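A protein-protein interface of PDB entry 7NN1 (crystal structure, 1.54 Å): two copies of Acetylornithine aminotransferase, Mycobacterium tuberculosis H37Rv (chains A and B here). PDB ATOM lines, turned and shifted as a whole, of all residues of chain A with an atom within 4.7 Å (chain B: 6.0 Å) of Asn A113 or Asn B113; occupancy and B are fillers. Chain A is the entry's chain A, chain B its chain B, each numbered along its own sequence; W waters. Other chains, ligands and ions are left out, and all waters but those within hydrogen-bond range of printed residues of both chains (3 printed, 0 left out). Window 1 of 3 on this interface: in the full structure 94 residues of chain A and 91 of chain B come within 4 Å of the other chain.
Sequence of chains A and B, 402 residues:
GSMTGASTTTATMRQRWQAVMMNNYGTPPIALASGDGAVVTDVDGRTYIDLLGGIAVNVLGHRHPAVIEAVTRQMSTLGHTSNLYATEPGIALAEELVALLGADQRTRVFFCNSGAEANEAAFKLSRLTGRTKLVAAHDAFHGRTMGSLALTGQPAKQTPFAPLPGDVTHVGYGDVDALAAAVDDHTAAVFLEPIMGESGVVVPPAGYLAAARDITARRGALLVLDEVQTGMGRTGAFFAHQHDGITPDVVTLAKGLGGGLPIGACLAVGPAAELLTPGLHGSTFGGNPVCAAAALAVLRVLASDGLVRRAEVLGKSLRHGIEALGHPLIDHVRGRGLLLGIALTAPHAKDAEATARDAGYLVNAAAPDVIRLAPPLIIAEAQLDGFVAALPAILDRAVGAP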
ATOM      1  N   CYS A 112     -28.272  29.531 -17.670  1.00  0.00           N
ATOM      2  CA  CYS A 112     -27.641  28.295 -18.130  1.00  0.00           C
ATOM      3  C   CYS A 112     -26.241  28.653 -18.612  1.00  0.00           C
ATOM      4  O   CYS A 112     -25.703  29.707 -18.257  1.00  0.00           O
ATOM      5  CB  CYS A 112     -28.511  27.602 -19.190  1.00  0.00           C
ATOM      6  SG  CYS A 112     -28.934  28.737 -20.541  1.00  0.00           S
ATOM      7  N   ASN A 113     -25.653  27.806 -19.469  1.00  0.00           N
ATOM      8  CA  ASN A 113     -24.240  27.986 -19.787  1.00  0.00           C
ATOM      9  C   ASN A 113     -23.941  28.344 -21.222  1.00  0.00           C
ATOM     10  O   ASN A 113     -22.767  28.573 -21.530  1.00  0.00           O
ATOM     11  CB  ASN A 113     -23.431  26.726 -19.483  1.00  0.00           C
ATOM     12  CG  ASN A 113     -23.623  26.259 -18.091  1.00  0.00           C
ATOM     13  OD1 ASN A 113     -23.148  26.897 -17.148  1.00  0.00           O
ATOM     14  ND2 ASN A 113     -24.348  25.145 -17.932  1.00  0.00           N
ATOM     15  N   SER A 114     -24.934  28.367 -22.103  1.00  0.00           N
ATOM     16  CA  SER A 114     -24.641  28.510 -23.522  1.00  0.00           C
ATOM     17  C   SER A 114     -25.882  29.000 -24.254  1.00  0.00           C
ATOM     18  O   SER A 114     -26.989  28.984 -23.722  1.00  0.00           O
ATOM     19  CB  SER A 114     -24.160  27.188 -24.126  1.00  0.00           C
ATOM     20  OG  SER A 114     -25.191  26.204 -24.076  1.00  0.00           O
ATOM     21  N   GLU A 117     -28.164  25.984 -24.808  1.00  0.00           N
ATOM     22  CA  GLU A 117     -28.939  25.675 -23.605  1.00  0.00           C
ATOM     23  C   GLU A 117     -30.029  26.711 -23.355  1.00  0.00           C
ATOM     24  O   GLU A 117     -31.104  26.369 -22.860  1.00  0.00           O
ATOM     25  CB  GLU A 117     -28.017  25.586 -22.378  1.00  0.00           C
ATOM     26  CG  GLU A 117     -27.231  24.285 -22.301  1.00  0.00           C
ATOM     27  CD  GLU A 117     -26.485  24.106 -20.978  1.00  0.00           C
ATOM     28  OE1 GLU A 117     -26.343  25.084 -20.226  1.00  0.00           O
ATOM     29  OE2 GLU A 117     -26.052  22.975 -20.678  1.00  0.00           O
ATOM     30  N   PRO A 262     -18.478  31.488 -19.534  1.00  0.00           N
ATOM     31  CA  PRO A 262     -19.664  30.812 -20.092  1.00  0.00           C
ATOM     32  C   PRO A 262     -20.896  31.079 -19.239  1.00  0.00           C
ATOM     33  O   PRO A 262     -20.936  30.740 -18.053  1.00  0.00           O
ATOM     34  CB  PRO A 262     -19.277  29.323 -20.084  1.00  0.00           C
ATOM     35  CG  PRO A 262     -17.785  29.292 -19.870  1.00  0.00           C
ATOM     36  CD  PRO A 262     -17.452  30.538 -19.078  1.00  0.00           C
ATOM     37  N   ILE A 263     -21.908  31.681 -19.862  1.00  0.00           N
ATOM     38  CA  ILE A 263     -23.191  31.941 -19.221  1.00  0.00           C
ATOM     39  C   ILE A 263     -24.194  32.270 -20.319  1.00  0.00           C
ATOM     40  O   ILE A 263     -23.863  32.941 -21.306  1.00  0.00           O
ATOM     41  CB  ILE A 263     -23.088  33.068 -18.160  1.00  0.00           C
ATOM     42  CG1 ILE A 263     -24.452  33.384 -17.564  1.00  0.00           C
ATOM     43  CG2 ILE A 263     -22.481  34.354 -18.739  1.00  0.00           C
ATOM     44  CD1 ILE A 263     -24.380  34.171 -16.247  1.00  0.00           C
ATOM     45  N   GLY A 264     -25.411  31.745 -20.156  1.00  0.00           N
ATOM     46  CA  GLY A 264     -26.523  32.094 -21.010  1.00  0.00           C
ATOM     47  C   GLY A 264     -27.753  32.369 -20.166  1.00  0.00           C
ATOM     48  O   GLY A 264     -27.778  32.087 -18.964  1.00  0.00           O
ATOM     49  N   SER A 283     -30.149  23.468 -14.536  1.00  0.00           N
ATOM     50  CA  SER A 283     -28.793  23.317 -15.047  1.00  0.00           C
ATOM     51  C   SER A 283     -27.843  23.466 -13.869  1.00  0.00           C
ATOM     52  O   SER A 283     -27.911  24.476 -13.161  1.00  0.00           O
ATOM     53  CB  SER A 283     -28.481  24.369 -16.131  1.00  0.00           C
ATOM     54  OG  SER A 283     -27.199  24.152 -16.711  1.00  0.00           O
ATOM     55  N   PHE A 285     -24.643  24.210 -13.277  1.00  0.00           N
ATOM     56  CA  PHE A 285     -23.822  25.419 -13.193  1.00  0.00           C
ATOM     57  C   PHE A 285     -24.604  26.713 -13.377  1.00  0.00           C
ATOM     58  O   PHE A 285     -23.998  27.783 -13.281  1.00  0.00           O
ATOM     59  CB  PHE A 285     -22.742  25.426 -14.281  1.00  0.00           C
ATOM     60  CG  PHE A 285     -21.778  24.282 -14.244  1.00  0.00           C
ATOM     61  CD1 PHE A 285     -21.153  23.889 -13.063  1.00  0.00           C
ATOM     62  CD2 PHE A 285     -21.453  23.625 -15.428  1.00  0.00           C
ATOM     63  CE1 PHE A 285     -20.229  22.852 -13.063  1.00  0.00           C
ATOM     64  CE2 PHE A 285     -20.535  22.591 -15.438  1.00  0.00           C
ATOM     65  CZ  PHE A 285     -19.924  22.192 -14.258  1.00  0.00           C
ATOM     66  N   GLY A 286     -25.886  26.660 -13.728  1.00  0.00           N
ATOM     67  CA  GLY A 286     -26.585  27.874 -14.138  1.00  0.00           C
ATOM     68  C   GLY A 286     -26.658  28.903 -13.028  1.00  0.00           C
ATOM     69  O   GLY A 286     -26.957  28.548 -11.884  1.00  0.00           O
ATOM     70  N   PHE B 111     -14.976  19.380 -25.996  1.00  0.00           N
ATOM     71  CA  PHE B 111     -15.320  20.150 -24.811  1.00  0.00           C
ATOM     72  C   PHE B 111     -16.635  20.904 -24.991  1.00  0.00           C
ATOM     73  O   PHE B 111     -16.997  21.338 -26.091  1.00  0.00           O
ATOM     74  CB  PHE B 111     -14.211  21.154 -24.474  1.00  0.00           C
ATOM     75  CG  PHE B 111     -12.955  20.517 -23.941  1.00  0.00           C
ATOM     76  CD1 PHE B 111     -12.979  19.767 -22.776  1.00  0.00           C
ATOM     77  CD2 PHE B 111     -11.740  20.709 -24.592  1.00  0.00           C
ATOM     78  CE1 PHE B 111     -11.826  19.182 -22.287  1.00  0.00           C
ATOM     79  CE2 PHE B 111     -10.581  20.144 -24.098  1.00  0.00           C
ATOM     80  CZ  PHE B 111     -10.626  19.372 -22.939  1.00  0.00           C
ATOM     81  N   CYS B 112     -17.323  21.101 -23.872  1.00  0.00           N
ATOM     82  CA  CYS B 112     -18.568  21.864 -23.860  1.00  0.00           C
ATOM     83  C   CYS B 112     -18.693  22.465 -22.467  1.00  0.00           C
ATOM     84  O   CYS B 112     -17.698  22.587 -21.748  1.00  0.00           O
ATOM     85  CB  CYS B 112     -19.765  20.970 -24.237  1.00  0.00           C
ATOM     86  SG  CYS B 112     -19.864  19.411 -23.296  1.00  0.00           S
ATOM     87  N   ASN B 113     -19.915  22.773 -22.062  1.00  0.00           N
ATOM     88  CA  ASN B 113     -20.138  23.562 -20.861  1.00  0.00           C
ATOM     89  C   ASN B 113     -20.865  22.862 -19.736  1.00  0.00           C
ATOM     90  O   ASN B 113     -20.965  23.447 -18.653  1.00  0.00           O
ATOM     91  CB  ASN B 113     -20.949  24.813 -21.189  1.00  0.00           C
ATOM     92  CG  ASN B 113     -20.288  25.648 -22.212  1.00  0.00           C
ATOM     93  OD1 ASN B 113     -19.276  26.293 -21.932  1.00  0.00           O
ATOM     94  ND2 ASN B 113     -20.821  25.620 -23.436  1.00  0.00           N
ATOM     95  N   SER B 114     -21.423  21.677 -19.948  1.00  0.00           N
ATOM     96  CA  SER B 114     -22.302  21.096 -18.945  1.00  0.00           C
ATOM     97  C   SER B 114     -22.368  19.596 -19.168  1.00  0.00           C
ATOM     98  O   SER B 114     -21.934  19.077 -20.202  1.00  0.00           O
ATOM     99  CB  SER B 114     -23.700  21.710 -19.019  1.00  0.00           C
ATOM    100  OG  SER B 114     -24.338  21.372 -20.246  1.00  0.00           O
ATOM    101  N   GLY B 115     -22.944  18.898 -18.188  1.00  0.00           N
ATOM    102  CA  GLY B 115     -23.164  17.470 -18.364  1.00  0.00           C
ATOM    103  C   GLY B 115     -24.213  17.165 -19.410  1.00  0.00           C
ATOM    104  O   GLY B 115     -24.067  16.219 -20.196  1.00  0.00           O
ATOM    105  N   GLU B 117     -24.819  18.973 -22.028  1.00  0.00           N
ATOM    106  CA  GLU B 117     -24.190  19.157 -23.335  1.00  0.00           C
ATOM    107  C   GLU B 117     -23.237  18.016 -23.664  1.00  0.00           C
ATOM    108  O   GLU B 117     -23.102  17.643 -24.835  1.00  0.00           O
ATOM    109  CB  GLU B 117     -23.447  20.494 -23.399  1.00  0.00           C
ATOM    110  CG  GLU B 117     -24.364  21.672 -23.562  1.00  0.00           C
ATOM    111  CD  GLU B 117     -23.610  22.964 -23.838  1.00  0.00           C
ATOM    112  OE1 GLU B 117     -22.373  23.022 -23.623  1.00  0.00           O
ATOM    113  OE2 GLU B 117     -24.261  23.932 -24.283  1.00  0.00           O
ATOM    114  N   ALA B 118     -22.521  17.489 -22.664  1.00  0.00           N
ATOM    115  CA  ALA B 118     -21.622  16.369 -22.933  1.00  0.00           C
ATOM    116  C   ALA B 118     -22.405  15.158 -23.416  1.00  0.00           C
ATOM    117  O   ALA B 118     -21.994  14.471 -24.366  1.00  0.00           O
ATOM    118  CB  ALA B 118     -20.809  16.026 -21.684  1.00  0.00           C
ATOM    119  N   ALA B 254     -18.445  16.279 -16.402  1.00  0.00           N
ATOM    120  CA  ALA B 254     -18.806  17.686 -16.114  1.00  0.00           C
ATOM    121  C   ALA B 254     -18.726  17.870 -14.604  1.00  0.00           C
ATOM    122  O   ALA B 254     -17.835  17.349 -14.026  1.00  0.00           O
ATOM    123  CB  ALA B 254     -20.156  18.137 -16.638  1.00  0.00           C
ATOM    124  N1  LLP B 255     -25.448  13.304 -15.863  1.00  0.00           N
ATOM    125  C2  LLP B 255     -25.275  13.072 -14.575  1.00  0.00           C
ATOM    126  C2' LLP B 255     -24.995  11.684 -14.112  1.00  0.00           C
ATOM    127  C3  LLP B 255     -25.327  14.115 -13.661  1.00  0.00           C
ATOM    128  O3  LLP B 255     -25.175  13.787 -12.386  1.00  0.00           O
ATOM    129  C4  LLP B 255     -25.584  15.425 -14.088  1.00  0.00           C
ATOM    130  C4' LLP B 255     -25.591  16.490 -13.089  1.00  0.00           C
ATOM    131  C5  LLP B 255     -25.773  15.635 -15.457  1.00  0.00           C
ATOM    132  C6  LLP B 255     -25.696  14.553 -16.281  1.00  0.00           C
ATOM    133  C5' LLP B 255     -26.146  16.964 -16.049  1.00  0.00           C
ATOM    134  OP4 LLP B 255     -25.251  18.054 -15.767  1.00  0.00           O
ATOM    135  P   LLP B 255     -25.647  19.541 -16.060  1.00  0.00           P
ATOM    136  OP1 LLP B 255     -24.387  20.256 -16.038  1.00  0.00           O
ATOM    137  OP2 LLP B 255     -26.333  19.629 -17.326  1.00  0.00           O
ATOM    138  OP3 LLP B 255     -26.527  19.866 -14.938  1.00  0.00           O
ATOM    139  N   LLP B 255     -19.684  18.576 -14.040  1.00  0.00           N
ATOM    140  CA  LLP B 255     -19.732  18.866 -12.583  1.00  0.00           C
ATOM    141  CB  LLP B 255     -20.478  17.776 -11.813  1.00  0.00           C
ATOM    142  CG  LLP B 255     -21.979  17.845 -12.022  1.00  0.00           C
ATOM    143  CD  LLP B 255     -22.835  17.005 -11.093  1.00  0.00           C
ATOM    144  CE  LLP B 255     -24.317  17.317 -11.232  1.00  0.00           C
ATOM    145  NZ  LLP B 255     -25.034  16.286 -11.967  1.00  0.00           N
ATOM    146  C   LLP B 255     -18.364  19.263 -12.019  1.00  0.00           C
ATOM    147  O   LLP B 255     -17.938  20.335 -12.261  1.00  0.00           O
ATOM    148  N   PRO B 262     -17.688  26.301 -15.173  1.00  0.00           N
ATOM    149  CA  PRO B 262     -18.521  25.456 -16.054  1.00  0.00           C
ATOM    150  C   PRO B 262     -17.707  24.859 -17.193  1.00  0.00           C
ATOM    151  O   PRO B 262     -17.186  25.581 -18.046  1.00  0.00           O
ATOM    152  CB  PRO B 262     -19.593  26.417 -16.586  1.00  0.00           C
ATOM    153  CG  PRO B 262     -19.368  27.749 -15.885  1.00  0.00           C
ATOM    154  CD  PRO B 262     -17.986  27.735 -15.289  1.00  0.00           C
ATOM    155  N   ILE B 263     -17.654  23.532 -17.231  1.00  0.00           N
ATOM    156  CA  ILE B 263     -16.968  22.826 -18.305  1.00  0.00           C
ATOM    157  C   ILE B 263     -17.436  21.381 -18.286  1.00  0.00           C
ATOM    158  O   ILE B 263     -17.688  20.803 -17.222  1.00  0.00           O
ATOM    159  CB  ILE B 263     -15.430  22.942 -18.166  1.00  0.00           C
ATOM    160  CG1 ILE B 263     -14.709  22.136 -19.247  1.00  0.00           C
ATOM    161  CG2 ILE B 263     -14.961  22.548 -16.751  1.00  0.00           C
ATOM    162  CD1 ILE B 263     -13.220  22.476 -19.342  1.00  0.00           C
ATOM    163  N   GLY B 264     -17.579  20.813 -19.484  1.00  0.00           N
ATOM    164  CA  GLY B 264     -17.885  19.410 -19.637  1.00  0.00           C
ATOM    165  C   GLY B 264     -17.045  18.851 -20.767  1.00  0.00           C
ATOM    166  O   GLY B 264     -16.429  19.603 -21.520  1.00  0.00           O
ATOM    167  N   SER B 283     -19.521  24.093 -29.987  1.00  0.00           N
ATOM    168  CA  SER B 283     -20.034  24.865 -28.858  1.00  0.00           C
ATOM    169  C   SER B 283     -19.150  26.101 -28.712  1.00  0.00           C
ATOM    170  O   SER B 283     -17.927  25.968 -28.606  1.00  0.00           O
ATOM    171  CB  SER B 283     -20.017  24.021 -27.571  1.00  0.00           C
ATOM    172  OG  SER B 283     -20.529  24.756 -26.476  1.00  0.00           O
ATOM    173  N   THR B 284     -19.752  27.296 -28.730  1.00  0.00           N
ATOM    174  CA  THR B 284     -18.956  28.529 -28.736  1.00  0.00           C
ATOM    175  C   THR B 284     -17.946  28.564 -27.592  1.00  0.00           C
ATOM    176  O   THR B 284     -16.752  28.793 -27.814  1.00  0.00           O
ATOM    177  CB  THR B 284     -19.865  29.755 -28.655  1.00  0.00           C
ATOM    178  OG1 THR B 284     -20.710  29.790 -29.809  1.00  0.00           O
ATOM    179  CG2 THR B 284     -19.017  31.051 -28.598  1.00  0.00           C
ATOM    180  N   PHE B 285     -18.408  28.324 -26.358  1.00  0.00           N
ATOM    181  CA  PHE B 285     -17.528  28.418 -25.198  1.00  0.00           C
ATOM    182  C   PHE B 285     -16.673  27.173 -24.978  1.00  0.00           C
ATOM    183  O   PHE B 285     -15.791  27.201 -24.115  1.00  0.00           O
ATOM    184  CB  PHE B 285     -18.332  28.639 -23.914  1.00  0.00           C
ATOM    185  CG  PHE B 285     -19.150  29.899 -23.878  1.00  0.00           C
ATOM    186  CD1 PHE B 285     -18.619  31.128 -24.264  1.00  0.00           C
ATOM    187  CD2 PHE B 285     -20.458  29.852 -23.390  1.00  0.00           C
ATOM    188  CE1 PHE B 285     -19.383  32.292 -24.179  1.00  0.00           C
ATOM    189  CE2 PHE B 285     -21.229  30.994 -23.296  1.00  0.00           C
ATOM    190  CZ  PHE B 285     -20.695  32.230 -23.697  1.00  0.00           C
ATOM    191  N   GLY B 286     -16.903  26.082 -25.716  1.00  0.00           N
ATOM    192  CA  GLY B 286     -16.212  24.843 -25.394  1.00  0.00           C
ATOM    193  C   GLY B 286     -14.700  24.942 -25.436  1.00  0.00           C
ATOM    194  O   GLY B 286     -14.120  25.465 -26.402  1.00  0.00           O
ATOM    195  N   ASN B 288     -12.670  26.717 -23.562  1.00  0.00           N
ATOM    196  CA  ASN B 288     -12.090  28.040 -23.460  1.00  0.00           C
ATOM    197  C   ASN B 288     -10.961  28.050 -22.427  1.00  0.00           C
ATOM    198  O   ASN B 288     -10.957  27.245 -21.477  1.00  0.00           O
ATOM    199  CB  ASN B 288     -13.152  29.073 -23.107  1.00  0.00           C
ATOM    200  CG  ASN B 288     -13.634  28.943 -21.682  1.00  0.00           C
ATOM    201  OD1 ASN B 288     -13.055  29.520 -20.753  1.00  0.00           O
ATOM    202  ND2 ASN B 288     -14.705  28.198 -21.500  1.00  0.00           N
HETATM  203  O   HOH W   1     -23.353  24.840 -26.686  1.00  0.00           O
HETATM  204  O   HOH W   2     -24.687  23.066 -15.856  1.00  0.00           O
HETATM  205  O   HOH W   3     -27.166  21.922 -18.469  1.00  0.00           O
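The side-chain hydroxyl of Ser A114 is in hydrogen-bond range of the side-chain carboxylate of Glu B117, at 2.5 Å.
OE2 of Glu A117 lies close to OG of Ser B114, at 2.4 Å.
The side-chain sulfur (SG) of Cys A112 sits at hydrogen-bond distance from the backbone carbonyl oxygen (O) of Ser A114 (3.7 Å).
N of Asn A113 sits at hydrogen-bond distance from OE1 of Glu A117, 2.9 Å away.
O of Ser B114 sits at hydrogen-bond distance from SG of Cys B112, 3.7 Å away.
N of Asn B113 sits at hydrogen-bond distance from OE1 of Glu B117 (2.9 Å).
The side-chain amide nitrogen (ND2) of Asn B113 sits at hydrogen-bond distance from the side-chain hydroxyl (OG) of Ser B283, 3.2 Å away.
The side-chain hydroxyl (OG) of Ser B114 sits at hydrogen-bond distance from the backbone NH (N) of Glu B117.
Among the printed residues, pairs that only touch across the chains: Asn A113 with Phe B285 (3.2 Å), Phe A285 with Asn B113 (3.3 Å), Phe A285 with LLP B255 (3.4 Å), Phe A285 with Pro B262 (3.5 Å), Phe A285 with Ile B263 (3.5 Å), Pro A262 with Phe B285 (3.5 Å), Pro A262 with Asn B113 (3.5 Å), Ile A263 with Phe B285 (3.6 Å), Asn A113 with Asn B113 (3.6 Å), Glu A117 with Glu B117 (3.6 Å), Asn A113 with Pro B262 (3.6 Å), Pro A262 with Asn B288 (3.7 Å), Asn A113 with Ser B114 (3.7 Å), Ser A114 with Asn B113 (3.8 Å) and Ser A283 with LLP B255 (3.98 Å).
Asn A113 touches just these residues of chain B: Asn B113 (3.6 Å), Ser B114 (3.7 Å), Pro B262 (3.6 Å) and Phe B285 (3.2 Å).
Of chain A, only Asn A113 (3.6 Å), Ser A114 (3.8 Å), Pro A262 (3.5 Å) and Phe A285 (3.3 Å) come within 4 Å of Asn B113.
Printed residues of chain A within 4 Å of Glu B117: Ser A114 and Glu A117.
Of the printed residues of chain B, Pro A262 touches Asn B113 (3.5 Å), Phe B285 (3.5 Å) and Asn B288 (3.7 Å).
Of the printed residues of chain A, Phe B285 touches Asn A113, Pro A262 and Ile A263.
Of the printed residues of chain B, Glu A117 touches Ser B114 (2.4 Å) and Glu B117 (3.6 Å).
Phe B111 touches none of the printed residues of chain A.
Ala B118 touches none of the printed residues of chain A.
The nearest residue of chain B that does not touch Asn A113 is LLP B255 (5.2 Å).
The nearest printed residue of chain A that does not touch Asn B113 is Glu A117 (5.3 Å).
The nearest printed residue of chain A that does not touch Glu B117 is Asn A113 (5.4 Å).
Of the 17 printed residues of chain B, 8 touch a printed residue of chain A.
Hydrophobic or aromatic side chains of chain A within 4 Å of the printed part of chain B: Pro A262 and Phe A285.
Among the printed residues, 17 pairs touch across the chains.
Among the printed residues, no Asp or Glu carboxylate lies within 4 Å of a Lys or Arg side-chain nitrogen of the other chain.
Asn A113 touches Ser B114, and with the chains exchanged Ser A114 touches Asn B113.
Asn A113 touches Pro B262, and with the chains exchanged Pro A262 touches Asn B113.
Glu B117 touches its own counterpart, Glu A117.
Pro A262 touches Phe B285, and with the chains exchanged Phe A285 touches Pro B262.
10 positions are printed for both chains.
Of the 17 pairs that touch across the chains among the printed residues, 14 have their exchanged pair printed and touching as well.
Water W3 lies within hydrogen-bond range of OE2 of Glu A117, OP2 of LLP B255, OG of Ser A283 and OG of Ser B114.
Water W1 lies within hydrogen-bond range of the side-chain carboxylate of Glu B117 (2.7 Å), the side-chain hydroxyl of Ser B283 (2.8 Å) and the side-chain hydroxyl of Ser A114 (3.5 Å).
Water W2 lies within hydrogen-bond range of the backbone NH of Phe A285 (2.8 Å), OP1 of LLP B255 (2.8 Å), the side-chain hydroxyl of Ser A283 (2.9 Å) and the side-chain amide nitrogen of Asn A113 (3.0 Å).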
